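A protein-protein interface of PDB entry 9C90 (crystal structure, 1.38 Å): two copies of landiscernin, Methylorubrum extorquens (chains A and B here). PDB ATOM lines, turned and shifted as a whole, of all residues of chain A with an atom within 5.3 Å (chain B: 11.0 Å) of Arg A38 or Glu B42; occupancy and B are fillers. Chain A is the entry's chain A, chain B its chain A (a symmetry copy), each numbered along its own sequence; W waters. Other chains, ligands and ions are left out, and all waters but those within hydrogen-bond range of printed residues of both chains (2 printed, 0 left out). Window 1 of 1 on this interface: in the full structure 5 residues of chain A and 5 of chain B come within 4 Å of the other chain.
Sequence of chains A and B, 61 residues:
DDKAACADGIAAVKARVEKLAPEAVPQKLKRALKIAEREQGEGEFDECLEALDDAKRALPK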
ATOM      1  N   LEU A  33      -4.820 -13.136  11.173  1.00  0.00           N
ATOM      2  CA  LEU A  33      -4.722 -12.946  12.616  1.00  0.00           C
ATOM      3  C   LEU A  33      -5.625 -13.922  13.350  1.00  0.00           C
ATOM      4  O   LEU A  33      -5.225 -14.501  14.362  1.00  0.00           O
ATOM      5  CB  LEU A  33      -5.098 -11.508  12.981  1.00  0.00           C
ATOM      6  CG  LEU A  33      -3.954 -10.541  13.260  1.00  0.00           C
ATOM      7  CD1 LEU A  33      -4.516  -9.186  13.669  1.00  0.00           C
ATOM      8  CD2 LEU A  33      -3.027 -11.095  14.341  1.00  0.00           C
ATOM      9  N   LYS A  34      -6.851 -14.122  12.849  1.00  0.00           N
ATOM     10  CA  LYS A  34      -7.771 -15.048  13.501  1.00  0.00           C
ATOM     11  C   LYS A  34      -7.251 -16.476  13.442  1.00  0.00           C
ATOM     12  O   LYS A  34      -7.416 -17.237  14.404  1.00  0.00           O
ATOM     13  CB  LYS A  34      -9.144 -15.005  12.841  1.00  0.00           C
ATOM     14  CG  LYS A  34     -10.055 -13.840  13.175  1.00  0.00           C
ATOM     15  CD  LYS A  34     -11.339 -14.019  12.319  1.00  0.00           C
ATOM     16  CE  LYS A  34     -12.505 -13.182  12.692  1.00  0.00           C
ATOM     17  NZ  LYS A  34     -13.622 -13.400  11.761  1.00  0.00           N
ATOM     18  N   ILE A  35      -6.667 -16.871  12.306  1.00  0.00           N
ATOM     19  CA  ILE A  35      -6.061 -18.199  12.215  1.00  0.00           C
ATOM     20  C   ILE A  35      -4.943 -18.332  13.239  1.00  0.00           C
ATOM     21  O   ILE A  35      -4.882 -19.314  13.988  1.00  0.00           O
ATOM     22  CB  ILE A  35      -5.579 -18.505  10.782  1.00  0.00           C
ATOM     23  CG1 ILE A  35      -6.769 -18.630   9.816  1.00  0.00           C
ATOM     24  CG2 ILE A  35      -4.712 -19.771  10.756  1.00  0.00           C
ATOM     25  CD1 ILE A  35      -7.667 -19.838  10.045  1.00  0.00           C
ATOM     26  N   ALA A  36      -4.055 -17.328  13.307  1.00  0.00           N
ATOM     27  CA  ALA A  36      -2.976 -17.371  14.285  1.00  0.00           C
ATOM     28  C   ALA A  36      -3.536 -17.563  15.687  1.00  0.00           C
ATOM     29  O   ALA A  36      -3.050 -18.408  16.446  1.00  0.00           O
ATOM     30  CB  ALA A  36      -2.130 -16.101  14.213  1.00  0.00           C
ATOM     31  N   GLU A  37      -4.604 -16.834  16.014  1.00  0.00           N
ATOM     32  CA  GLU A  37      -5.175 -16.931  17.354  1.00  0.00           C
ATOM     33  C   GLU A  37      -5.822 -18.291  17.586  1.00  0.00           C
ATOM     34  O   GLU A  37      -5.713 -18.847  18.693  1.00  0.00           O
ATOM     35  CB  GLU A  37      -6.151 -15.782  17.592  1.00  0.00           C
ATOM     36  CG  GLU A  37      -5.436 -14.453  17.720  1.00  0.00           C
ATOM     37  CD  GLU A  37      -6.349 -13.265  17.456  1.00  0.00           C
ATOM     38  OE1 GLU A  37      -7.548 -13.481  17.223  1.00  0.00           O
ATOM     39  OE2 GLU A  37      -5.854 -12.114  17.493  1.00  0.00           O
ATOM     40  N   ARG A  38      -6.469 -18.854  16.558  1.00  0.00           N
ATOM     41  CA  ARG A  38      -7.043 -20.192  16.690  1.00  0.00           C
ATOM     42  C   ARG A  38      -5.954 -21.204  16.980  1.00  0.00           C
ATOM     43  O   ARG A  38      -6.082 -22.036  17.886  1.00  0.00           O
ATOM     44  CB  ARG A  38      -7.741 -20.609  15.406  1.00  0.00           C
ATOM     45  CG  ARG A  38      -8.339 -22.011  15.480  1.00  0.00           C
ATOM     46  CD  ARG A  38      -8.836 -22.464  14.120  1.00  0.00           C
ATOM     47  NE  ARG A  38      -7.711 -22.754  13.246  1.00  0.00           N
ATOM     48  CZ  ARG A  38      -7.806 -22.844  11.927  1.00  0.00           C
ATOM     49  NH1 ARG A  38      -8.966 -22.674  11.310  1.00  0.00           N
ATOM     50  NH2 ARG A  38      -6.714 -23.120  11.218  1.00  0.00           N
ATOM     51  N   GLU A  39      -4.870 -21.155  16.208  1.00  0.00           N
ATOM     52  CA  GLU A  39      -3.793 -22.111  16.384  1.00  0.00           C
ATOM     53  C   GLU A  39      -3.075 -21.904  17.714  1.00  0.00           C
ATOM     54  O   GLU A  39      -2.668 -22.876  18.358  1.00  0.00           O
ATOM     55  CB  GLU A  39      -2.848 -22.028  15.183  1.00  0.00           C
ATOM     56  CG  GLU A  39      -3.522 -22.508  13.896  1.00  0.00           C
ATOM     57  CD  GLU A  39      -4.038 -23.946  13.986  1.00  0.00           C
ATOM     58  OE1 GLU A  39      -3.288 -24.815  14.475  1.00  0.00           O
ATOM     59  OE2 GLU A  39      -5.193 -24.218  13.572  1.00  0.00           O
ATOM     60  N   GLN A  40      -2.917 -20.645  18.142  1.00  0.00           N
ATOM     61  CA  GLN A  40      -2.392 -20.378  19.480  1.00  0.00           C
ATOM     62  C   GLN A  40      -3.238 -21.078  20.534  1.00  0.00           C
ATOM     63  O   GLN A  40      -2.705 -21.747  21.425  1.00  0.00           O
ATOM     64  CB  GLN A  40      -2.350 -18.870  19.736  1.00  0.00           C
ATOM     65  CG  GLN A  40      -1.943 -18.508  21.142  1.00  0.00           C
ATOM     66  CD  GLN A  40      -2.034 -17.011  21.431  1.00  0.00           C
ATOM     67  OE1 GLN A  40      -1.086 -16.410  21.946  1.00  0.00           O
ATOM     68  NE2 GLN A  40      -3.181 -16.419  21.120  1.00  0.00           N
ATOM     69  N   GLY A  41      -4.566 -20.971  20.416  1.00  0.00           N
ATOM     70  CA  GLY A  41      -5.449 -21.575  21.398  1.00  0.00           C
ATOM     71  C   GLY A  41      -5.398 -23.085  21.391  1.00  0.00           C
ATOM     72  O   GLY A  41      -5.673 -23.722  22.410  1.00  0.00           O
ATOM     73  N   GLU A  42      -5.034 -23.677  20.259  1.00  0.00           N
ATOM     74  CA  GLU A  42      -4.878 -25.118  20.146  1.00  0.00           C
ATOM     75  C   GLU A  42      -3.520 -25.582  20.627  1.00  0.00           C
ATOM     76  O   GLU A  42      -3.263 -26.793  20.640  1.00  0.00           O
ATOM     77  CB  GLU A  42      -5.058 -25.534  18.684  1.00  0.00           C
ATOM     78  CG  GLU A  42      -6.450 -25.244  18.179  1.00  0.00           C
ATOM     79  CD  GLU A  42      -6.643 -25.546  16.710  1.00  0.00           C
ATOM     80  OE1 GLU A  42      -5.673 -25.878  15.998  1.00  0.00           O
ATOM     81  OE2 GLU A  42      -7.802 -25.427  16.285  1.00  0.00           O
ATOM     82  N   GLU A  44      -0.808 -24.923  19.006  1.00  0.00           N
ATOM     83  CA  GLU A  44       0.050 -25.063  17.835  1.00  0.00           C
ATOM     84  C   GLU A  44       0.763 -23.734  17.599  1.00  0.00           C
ATOM     85  O   GLU A  44       0.449 -22.975  16.679  1.00  0.00           O
ATOM     86  CB  GLU A  44      -0.775 -25.477  16.629  1.00  0.00           C
ATOM     87  CG  GLU A  44      -1.722 -26.634  16.887  1.00  0.00           C
ATOM     88  CD  GLU A  44      -2.067 -27.347  15.597  1.00  0.00           C
ATOM     89  OE1 GLU A  44      -1.107 -27.753  14.934  1.00  0.00           O
ATOM     90  OE2 GLU A  44      -3.269 -27.457  15.225  1.00  0.00           O
ATOM     91  N   LYS B   3      -5.102 -35.546   2.504  1.00  0.00           N
ATOM     92  CA  LYS B   3      -6.532 -35.344   2.712  1.00  0.00           C
ATOM     93  C   LYS B   3      -7.290 -36.662   2.642  1.00  0.00           C
ATOM     94  O   LYS B   3      -8.129 -36.961   3.503  1.00  0.00           O
ATOM     95  CB  LYS B   3      -7.091 -34.340   1.704  1.00  0.00           C
ATOM     96  CG  LYS B   3      -8.594 -34.160   1.834  1.00  0.00           C
ATOM     97  CD  LYS B   3      -9.111 -33.019   0.970  1.00  0.00           C
ATOM     98  CE  LYS B   3     -10.631 -32.918   1.015  1.00  0.00           C
ATOM     99  NZ  LYS B   3     -11.113 -31.810   0.174  1.00  0.00           N
ATOM    100  N   CYS B   6      -6.287 -38.821   5.623  1.00  0.00           N
ATOM    101  CA  CYS B   6      -6.937 -38.374   6.851  1.00  0.00           C
ATOM    102  C   CYS B   6      -8.374 -38.877   6.927  1.00  0.00           C
ATOM    103  O   CYS B   6      -8.800 -39.430   7.949  1.00  0.00           O
ATOM    104  CB  CYS B   6      -6.883 -36.849   6.951  1.00  0.00           C
ATOM    105  SG  CYS B   6      -7.969 -36.134   8.200  1.00  0.00           S
ATOM    106  N   ILE B  10      -9.683 -41.592   9.613  1.00  0.00           N
ATOM    107  CA  ILE B  10     -10.764 -41.337  10.562  1.00  0.00           C
ATOM    108  C   ILE B  10     -11.804 -42.444  10.486  1.00  0.00           C
ATOM    109  O   ILE B  10     -12.258 -42.965  11.511  1.00  0.00           O
ATOM    110  CB  ILE B  10     -11.384 -39.944  10.332  1.00  0.00           C
ATOM    111  CG1 ILE B  10     -10.388 -38.839  10.696  1.00  0.00           C
ATOM    112  CG2 ILE B  10     -12.659 -39.790  11.146  1.00  0.00           C
ATOM    113  CD1 ILE B  10     -10.853 -37.447  10.369  1.00  0.00           C
ATOM    114  N   LEU B  33      -9.503 -38.701  18.390  1.00  0.00           N
ATOM    115  CA  LEU B  33     -10.366 -38.676  17.214  1.00  0.00           C
ATOM    116  C   LEU B  33     -10.935 -37.285  16.994  1.00  0.00           C
ATOM    117  O   LEU B  33     -10.985 -36.804  15.859  1.00  0.00           O
ATOM    118  CB  LEU B  33     -11.502 -39.687  17.377  1.00  0.00           C
ATOM    119  CG  LEU B  33     -11.357 -41.017  16.647  1.00  0.00           C
ATOM    120  CD1 LEU B  33     -12.604 -41.863  16.871  1.00  0.00           C
ATOM    121  CD2 LEU B  33     -11.109 -40.795  15.156  1.00  0.00           C
ATOM    122  N   LYS B  34     -11.366 -36.618  18.073  1.00  0.00           N
ATOM    123  CA  LYS B  34     -11.921 -35.277  17.936  1.00  0.00           C
ATOM    124  C   LYS B  34     -10.872 -34.290  17.447  1.00  0.00           C
ATOM    125  O   LYS B  34     -11.183 -33.395  16.651  1.00  0.00           O
ATOM    126  CB  LYS B  34     -12.472 -34.778  19.267  1.00  0.00           C
ATOM    127  CG  LYS B  34     -13.818 -35.306  19.720  1.00  0.00           C
ATOM    128  CD  LYS B  34     -14.091 -34.689  21.120  1.00  0.00           C
ATOM    129  CE  LYS B  34     -15.476 -34.808  21.637  1.00  0.00           C
ATOM    130  NZ  LYS B  34     -15.575 -34.246  22.993  1.00  0.00           N
ATOM    131  N   ILE B  35      -9.638 -34.407  17.949  1.00  0.00           N
ATOM    132  CA  ILE B  35      -8.559 -33.554  17.452  1.00  0.00           C
ATOM    133  C   ILE B  35      -8.349 -33.796  15.964  1.00  0.00           C
ATOM    134  O   ILE B  35      -8.282 -32.849  15.171  1.00  0.00           O
ATOM    135  CB  ILE B  35      -7.262 -33.749  18.264  1.00  0.00           C
ATOM    136  CG1 ILE B  35      -7.434 -33.241  19.705  1.00  0.00           C
ATOM    137  CG2 ILE B  35      -6.077 -33.062  17.574  1.00  0.00           C
ATOM    138  CD1 ILE B  35      -7.598 -31.734  19.847  1.00  0.00           C
ATOM    139  N   ALA B  36      -8.268 -35.072  15.558  1.00  0.00           N
ATOM    140  CA  ALA B  36      -8.098 -35.381  14.145  1.00  0.00           C
ATOM    141  C   ALA B  36      -9.195 -34.722  13.321  1.00  0.00           C
ATOM    142  O   ALA B  36      -8.917 -34.092  12.295  1.00  0.00           O
ATOM    143  CB  ALA B  36      -8.089 -36.892  13.918  1.00  0.00           C
ATOM    144  N   GLU B  37     -10.438 -34.800  13.800  1.00  0.00           N
ATOM    145  CA  GLU B  37     -11.550 -34.229  13.048  1.00  0.00           C
ATOM    146  C   GLU B  37     -11.478 -32.707  13.016  1.00  0.00           C
ATOM    147  O   GLU B  37     -11.787 -32.095  11.979  1.00  0.00           O
ATOM    148  CB  GLU B  37     -12.877 -34.730  13.613  1.00  0.00           C
ATOM    149  CG  GLU B  37     -13.099 -36.197  13.314  1.00  0.00           C
ATOM    150  CD  GLU B  37     -14.110 -36.844  14.249  1.00  0.00           C
ATOM    151  OE1 GLU B  37     -14.671 -36.131  15.096  1.00  0.00           O
ATOM    152  OE2 GLU B  37     -14.342 -38.068  14.120  1.00  0.00           O
ATOM    153  N   ARG B  38     -11.046 -32.083  14.120  1.00  0.00           N
ATOM    154  CA  ARG B  38     -10.877 -30.632  14.129  1.00  0.00           C
ATOM    155  C   ARG B  38      -9.847 -30.216  13.099  1.00  0.00           C
ATOM    156  O   ARG B  38     -10.068 -29.286  12.315  1.00  0.00           O
ATOM    157  CB  ARG B  38     -10.400 -30.153  15.489  1.00  0.00           C
ATOM    158  CG  ARG B  38     -10.183 -28.643  15.549  1.00  0.00           C
ATOM    159  CD  ARG B  38      -9.511 -28.239  16.847  1.00  0.00           C
ATOM    160  NE  ARG B  38      -8.119 -28.659  16.843  1.00  0.00           N
ATOM    161  CZ  ARG B  38      -7.373 -28.751  17.935  1.00  0.00           C
ATOM    162  NH1 ARG B  38      -7.867 -28.456  19.129  1.00  0.00           N
ATOM    163  NH2 ARG B  38      -6.106 -29.140  17.821  1.00  0.00           N
ATOM    164  N   GLU B  39      -8.701 -30.894  13.093  1.00  0.00           N
ATOM    165  CA  GLU B  39      -7.638 -30.541  12.170  1.00  0.00           C
ATOM    166  C   GLU B  39      -8.031 -30.839  10.727  1.00  0.00           C
ATOM    167  O   GLU B  39      -7.678 -30.081   9.818  1.00  0.00           O
ATOM    168  CB  GLU B  39      -6.351 -31.252  12.592  1.00  0.00           C
ATOM    169  CG  GLU B  39      -5.826 -30.730  13.931  1.00  0.00           C
ATOM    170  CD  GLU B  39      -5.547 -29.225  13.924  1.00  0.00           C
ATOM    171  OE1 GLU B  39      -4.925 -28.743  12.956  1.00  0.00           O
ATOM    172  OE2 GLU B  39      -5.947 -28.515  14.881  1.00  0.00           O
ATOM    173  N   GLN B  40      -8.764 -31.936  10.500  1.00  0.00           N
ATOM    174  CA  GLN B  40      -9.318 -32.195   9.172  1.00  0.00           C
ATOM    175  C   GLN B  40     -10.165 -31.018   8.708  1.00  0.00           C
ATOM    176  O   GLN B  40     -10.014 -30.542   7.579  1.00  0.00           O
ATOM    177  CB  GLN B  40     -10.146 -33.481   9.190  1.00  0.00           C
ATOM    178  CG  GLN B  40     -10.862 -33.757   7.891  1.00  0.00           C
ATOM    179  CD  GLN B  40     -11.793 -34.965   7.959  1.00  0.00           C
ATOM    180  OE1 GLN B  40     -11.743 -35.848   7.096  1.00  0.00           O
ATOM    181  NE2 GLN B  40     -12.653 -34.992   8.971  1.00  0.00           N
ATOM    182  N   GLY B  41     -11.029 -30.507   9.591  1.00  0.00           N
ATOM    183  CA  GLY B  41     -11.904 -29.408   9.223  1.00  0.00           C
ATOM    184  C   GLY B  41     -11.158 -28.123   8.952  1.00  0.00           C
ATOM    185  O   GLY B  41     -11.634 -27.275   8.195  1.00  0.00           O
ATOM    186  N   GLU B  42      -9.981 -27.965   9.546  1.00  0.00           N
ATOM    187  CA  GLU B  42      -9.135 -26.807   9.309  1.00  0.00           C
ATOM    188  C   GLU B  42      -8.294 -26.962   8.061  1.00  0.00           C
ATOM    189  O   GLU B  42      -7.562 -26.029   7.703  1.00  0.00           O
ATOM    190  CB  GLU B  42      -8.210 -26.599  10.512  1.00  0.00           C
ATOM    191  CG  GLU B  42      -8.979 -26.281  11.770  1.00  0.00           C
ATOM    192  CD  GLU B  42      -8.112 -26.169  13.004  1.00  0.00           C
ATOM    193  OE1 GLU B  42      -6.897 -26.453  12.953  1.00  0.00           O
ATOM    194  OE2 GLU B  42      -8.691 -25.799  14.036  1.00  0.00           O
ATOM    195  N   GLY B  43      -8.369 -28.118   7.403  1.00  0.00           N
ATOM    196  CA  GLY B  43      -7.537 -28.402   6.257  1.00  0.00           C
ATOM    197  C   GLY B  43      -6.128 -28.788   6.608  1.00  0.00           C
ATOM    198  O   GLY B  43      -5.275 -28.837   5.722  1.00  0.00           O
ATOM    199  N   GLU B  44      -5.858 -29.071   7.885  1.00  0.00           N
ATOM    200  CA  GLU B  44      -4.541 -29.544   8.297  1.00  0.00           C
ATOM    201  C   GLU B  44      -4.552 -31.070   8.289  1.00  0.00           C
ATOM    202  O   GLU B  44      -4.582 -31.732   9.328  1.00  0.00           O
ATOM    203  CB  GLU B  44      -4.194 -28.995   9.670  1.00  0.00           C
ATOM    204  CG  GLU B  44      -4.431 -27.504   9.825  1.00  0.00           C
ATOM    205  CD  GLU B  44      -3.577 -26.935  10.938  1.00  0.00           C
ATOM    206  OE1 GLU B  44      -2.362 -27.142  10.842  1.00  0.00           O
ATOM    207  OE2 GLU B  44      -4.109 -26.336  11.914  1.00  0.00           O
ATOM    208  N   PHE B  45      -4.576 -31.619   7.070  1.00  0.00           N
ATOM    209  CA  PHE B  45      -4.748 -33.056   6.925  1.00  0.00           C
ATOM    210  C   PHE B  45      -3.531 -33.803   7.437  1.00  0.00           C
ATOM    211  O   PHE B  45      -3.654 -34.935   7.925  1.00  0.00           O
ATOM    212  CB  PHE B  45      -5.054 -33.389   5.469  1.00  0.00           C
ATOM    213  CG  PHE B  45      -6.249 -32.661   4.944  1.00  0.00           C
ATOM    214  CD1 PHE B  45      -7.510 -32.949   5.435  1.00  0.00           C
ATOM    215  CD2 PHE B  45      -6.110 -31.675   3.986  1.00  0.00           C
ATOM    216  CE1 PHE B  45      -8.615 -32.275   4.969  1.00  0.00           C
ATOM    217  CE2 PHE B  45      -7.213 -30.992   3.507  1.00  0.00           C
ATOM    218  CZ  PHE B  45      -8.471 -31.301   3.998  1.00  0.00           C
ATOM    219  N   ASP B  46      -2.363 -33.169   7.376  1.00  0.00           N
ATOM    220  CA  ASP B  46      -1.175 -33.767   7.966  1.00  0.00           C
ATOM    221  C   ASP B  46      -1.311 -33.873   9.483  1.00  0.00           C
ATOM    222  O   ASP B  46      -0.972 -34.912  10.069  1.00  0.00           O
ATOM    223  CB  ASP B  46       0.074 -32.990   7.539  1.00  0.00           C
ATOM    224  CG  ASP B  46      -0.128 -31.479   7.554  1.00  0.00           C
ATOM    225  OD1 ASP B  46      -1.113 -31.009   8.184  1.00  0.00           O
ATOM    226  OD2 ASP B  46       0.708 -30.769   6.936  1.00  0.00           O
ATOM    227  N   GLU B  47      -1.820 -32.827  10.136  1.00  0.00           N
ATOM    228  CA  GLU B  47      -1.979 -32.878  11.587  1.00  0.00           C
ATOM    229  C   GLU B  47      -3.058 -33.869  11.989  1.00  0.00           C
ATOM    230  O   GLU B  47      -2.984 -34.467  13.071  1.00  0.00           O
ATOM    231  CB  GLU B  47      -2.342 -31.498  12.118  1.00  0.00           C
ATOM    232  CG  GLU B  47      -1.416 -30.418  11.627  1.00  0.00           C
ATOM    233  CD  GLU B  47      -0.791 -29.661  12.755  1.00  0.00           C
ATOM    234  OE1 GLU B  47      -0.757 -30.207  13.877  1.00  0.00           O
ATOM    235  OE2 GLU B  47      -0.343 -28.519  12.521  1.00  0.00           O
ATOM    236  N   CYS B  48      -4.072 -34.037  11.141  1.00  0.00           N
ATOM    237  CA  CYS B  48      -5.060 -35.073  11.373  1.00  0.00           C
ATOM    238  C   CYS B  48      -4.393 -36.441  11.425  1.00  0.00           C
ATOM    239  O   CYS B  48      -4.687 -37.251  12.310  1.00  0.00           O
ATOM    240  CB  CYS B  48      -6.090 -35.016  10.243  1.00  0.00           C
ATOM    241  SG  CYS B  48      -7.086 -36.478  10.035  1.00  0.00           S
ATOM    242  N   LEU B  49      -3.447 -36.692  10.515  1.00  0.00           N
ATOM    243  CA  LEU B  49      -2.799 -37.998  10.480  1.00  0.00           C
ATOM    244  C   LEU B  49      -1.985 -38.246  11.743  1.00  0.00           C
ATOM    245  O   LEU B  49      -1.945 -39.372  12.252  1.00  0.00           O
ATOM    246  CB  LEU B  49      -1.940 -38.117   9.225  1.00  0.00           C
ATOM    247  CG  LEU B  49      -2.774 -38.196   7.943  1.00  0.00           C
ATOM    248  CD1 LEU B  49      -1.927 -37.881   6.748  1.00  0.00           C
ATOM    249  CD2 LEU B  49      -3.422 -39.561   7.771  1.00  0.00           C
ATOM    250  N   ALA B  51      -2.662 -36.982  14.734  1.00  0.00           N
ATOM    251  CA  ALA B  51      -3.637 -37.269  15.782  1.00  0.00           C
ATOM    252  C   ALA B  51      -4.212 -38.671  15.636  1.00  0.00           C
ATOM    253  O   ALA B  51      -4.506 -39.332  16.637  1.00  0.00           O
ATOM    254  CB  ALA B  51      -4.756 -36.232  15.764  1.00  0.00           C
HETATM  255  O   HOH W   1      -4.979 -28.640  20.537  1.00  0.00           O
HETATM  256  O   HOH W   2      -7.778 -23.638   8.480  1.00  0.00           O
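The side-chain carboxylate (OE2) of Glu B42 is in salt-bridge range of the guanidinium group (NE) of Arg A38, 3.3 Å away.
OE2 of Glu A42 is in salt-bridge range of NE of Arg B38 (3.3 Å).
The side-chain carboxylate (OE2) of Glu A42 sits close to the side-chain carboxylate (OE2) of Glu B42, 2.4 Å away.
The side-chain carboxylate (OE1) of Glu A44 sits close to the side-chain carboxylate (OE2) of Glu B47, at 2.6 Å.
The side-chain carboxylate (OE2) of Glu A39 lies close to the side-chain carboxylate (OE1) of Glu B42 (2.9 Å).
The side-chain carboxylate of Glu B44 lies close to the side-chain carboxylate of Glu A39.
The side-chain carboxylate (OE2) of Glu B39 sits close to the side-chain carboxylate (OE1) of Glu A42.
OE2 of Glu A44 lies close to OE2 of Glu B39 (2.9 Å).
The guanidinium group (NE) of Arg A38 is in salt-bridge range of the side-chain carboxylate (OE2) of Glu A39 (2.9 Å).
The backbone carbonyl oxygen (O) of Glu A39 sits at hydrogen-bond distance from the backbone NH (N) of Glu A44 (2.8 Å).
OE2 of Glu B39 is in salt-bridge range of NE of Arg B38.
The backbone carbonyl oxygen (O) of Glu B39 sits at hydrogen-bond distance from the backbone NH (N) of Glu B44, at 2.8 Å.
The side-chain sulfur (SG) of Cys B6 is disulfide-bonded to the side-chain sulfur (SG) of Cys B48, at 2.1 Å.
Among the printed residues, merely in contact across the chains: Glu A44 with Glu B44 (3.6 Å).
Of chain B, only Glu B42 (3.3 Å) comes within 4 Å of Arg A38.
Glu B42 touches just these residues of chain A: Arg A38, Glu A39 and Glu A42.
Of chain B, only Glu B42 and Glu B44 come within 4 Å of Glu A39.
No residue of chain B comes within 4 Å of Gly A41.
Of the printed residues of chain A, Glu B39 touches Glu A42 (2.9 Å) and Glu A44 (2.9 Å).
Of the printed residues of chain A, Glu B47 touches Glu A44.
Of the printed residues of chain A, Glu B44 touches Glu A39 and Glu A44.
Leu B49 touches none of the printed residues of chain A.
Phe B45 touches none of the printed residues of chain A.
The nearest residue of chain B that does not touch Arg A38 is Glu B44 (4.2 Å).
The nearest residue of chain A that does not touch Glu B42 is Glu A44 (4.4 Å).
Of the 21 printed residues of chain B, 5 touch a printed residue of chain A.
Among the printed residues, 9 pairs touch across the chains.
Glu A39 touches Glu B42, and with the chains exchanged Glu A42 touches Glu B39.
Glu A39 touches Glu B44, and with the chains exchanged Glu A44 touches Glu B39.
Glu B42 touches its own counterpart, Glu A42.
Glu B44 touches its own counterpart, Glu A44.
Positions printed for both chains: 33, 34, 35, 36, 37, 38, 39, 40, 41, 42 and 44.
Water W1 lies within hydrogen-bond range of O of Glu A42 (2.5 Å) and NH2 of Arg B38 (3.0 Å).
Water W2 lies within hydrogen-bond range of O of Glu B42 (2.5 Å) and NH2 of Arg A38 (3.0 Å).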
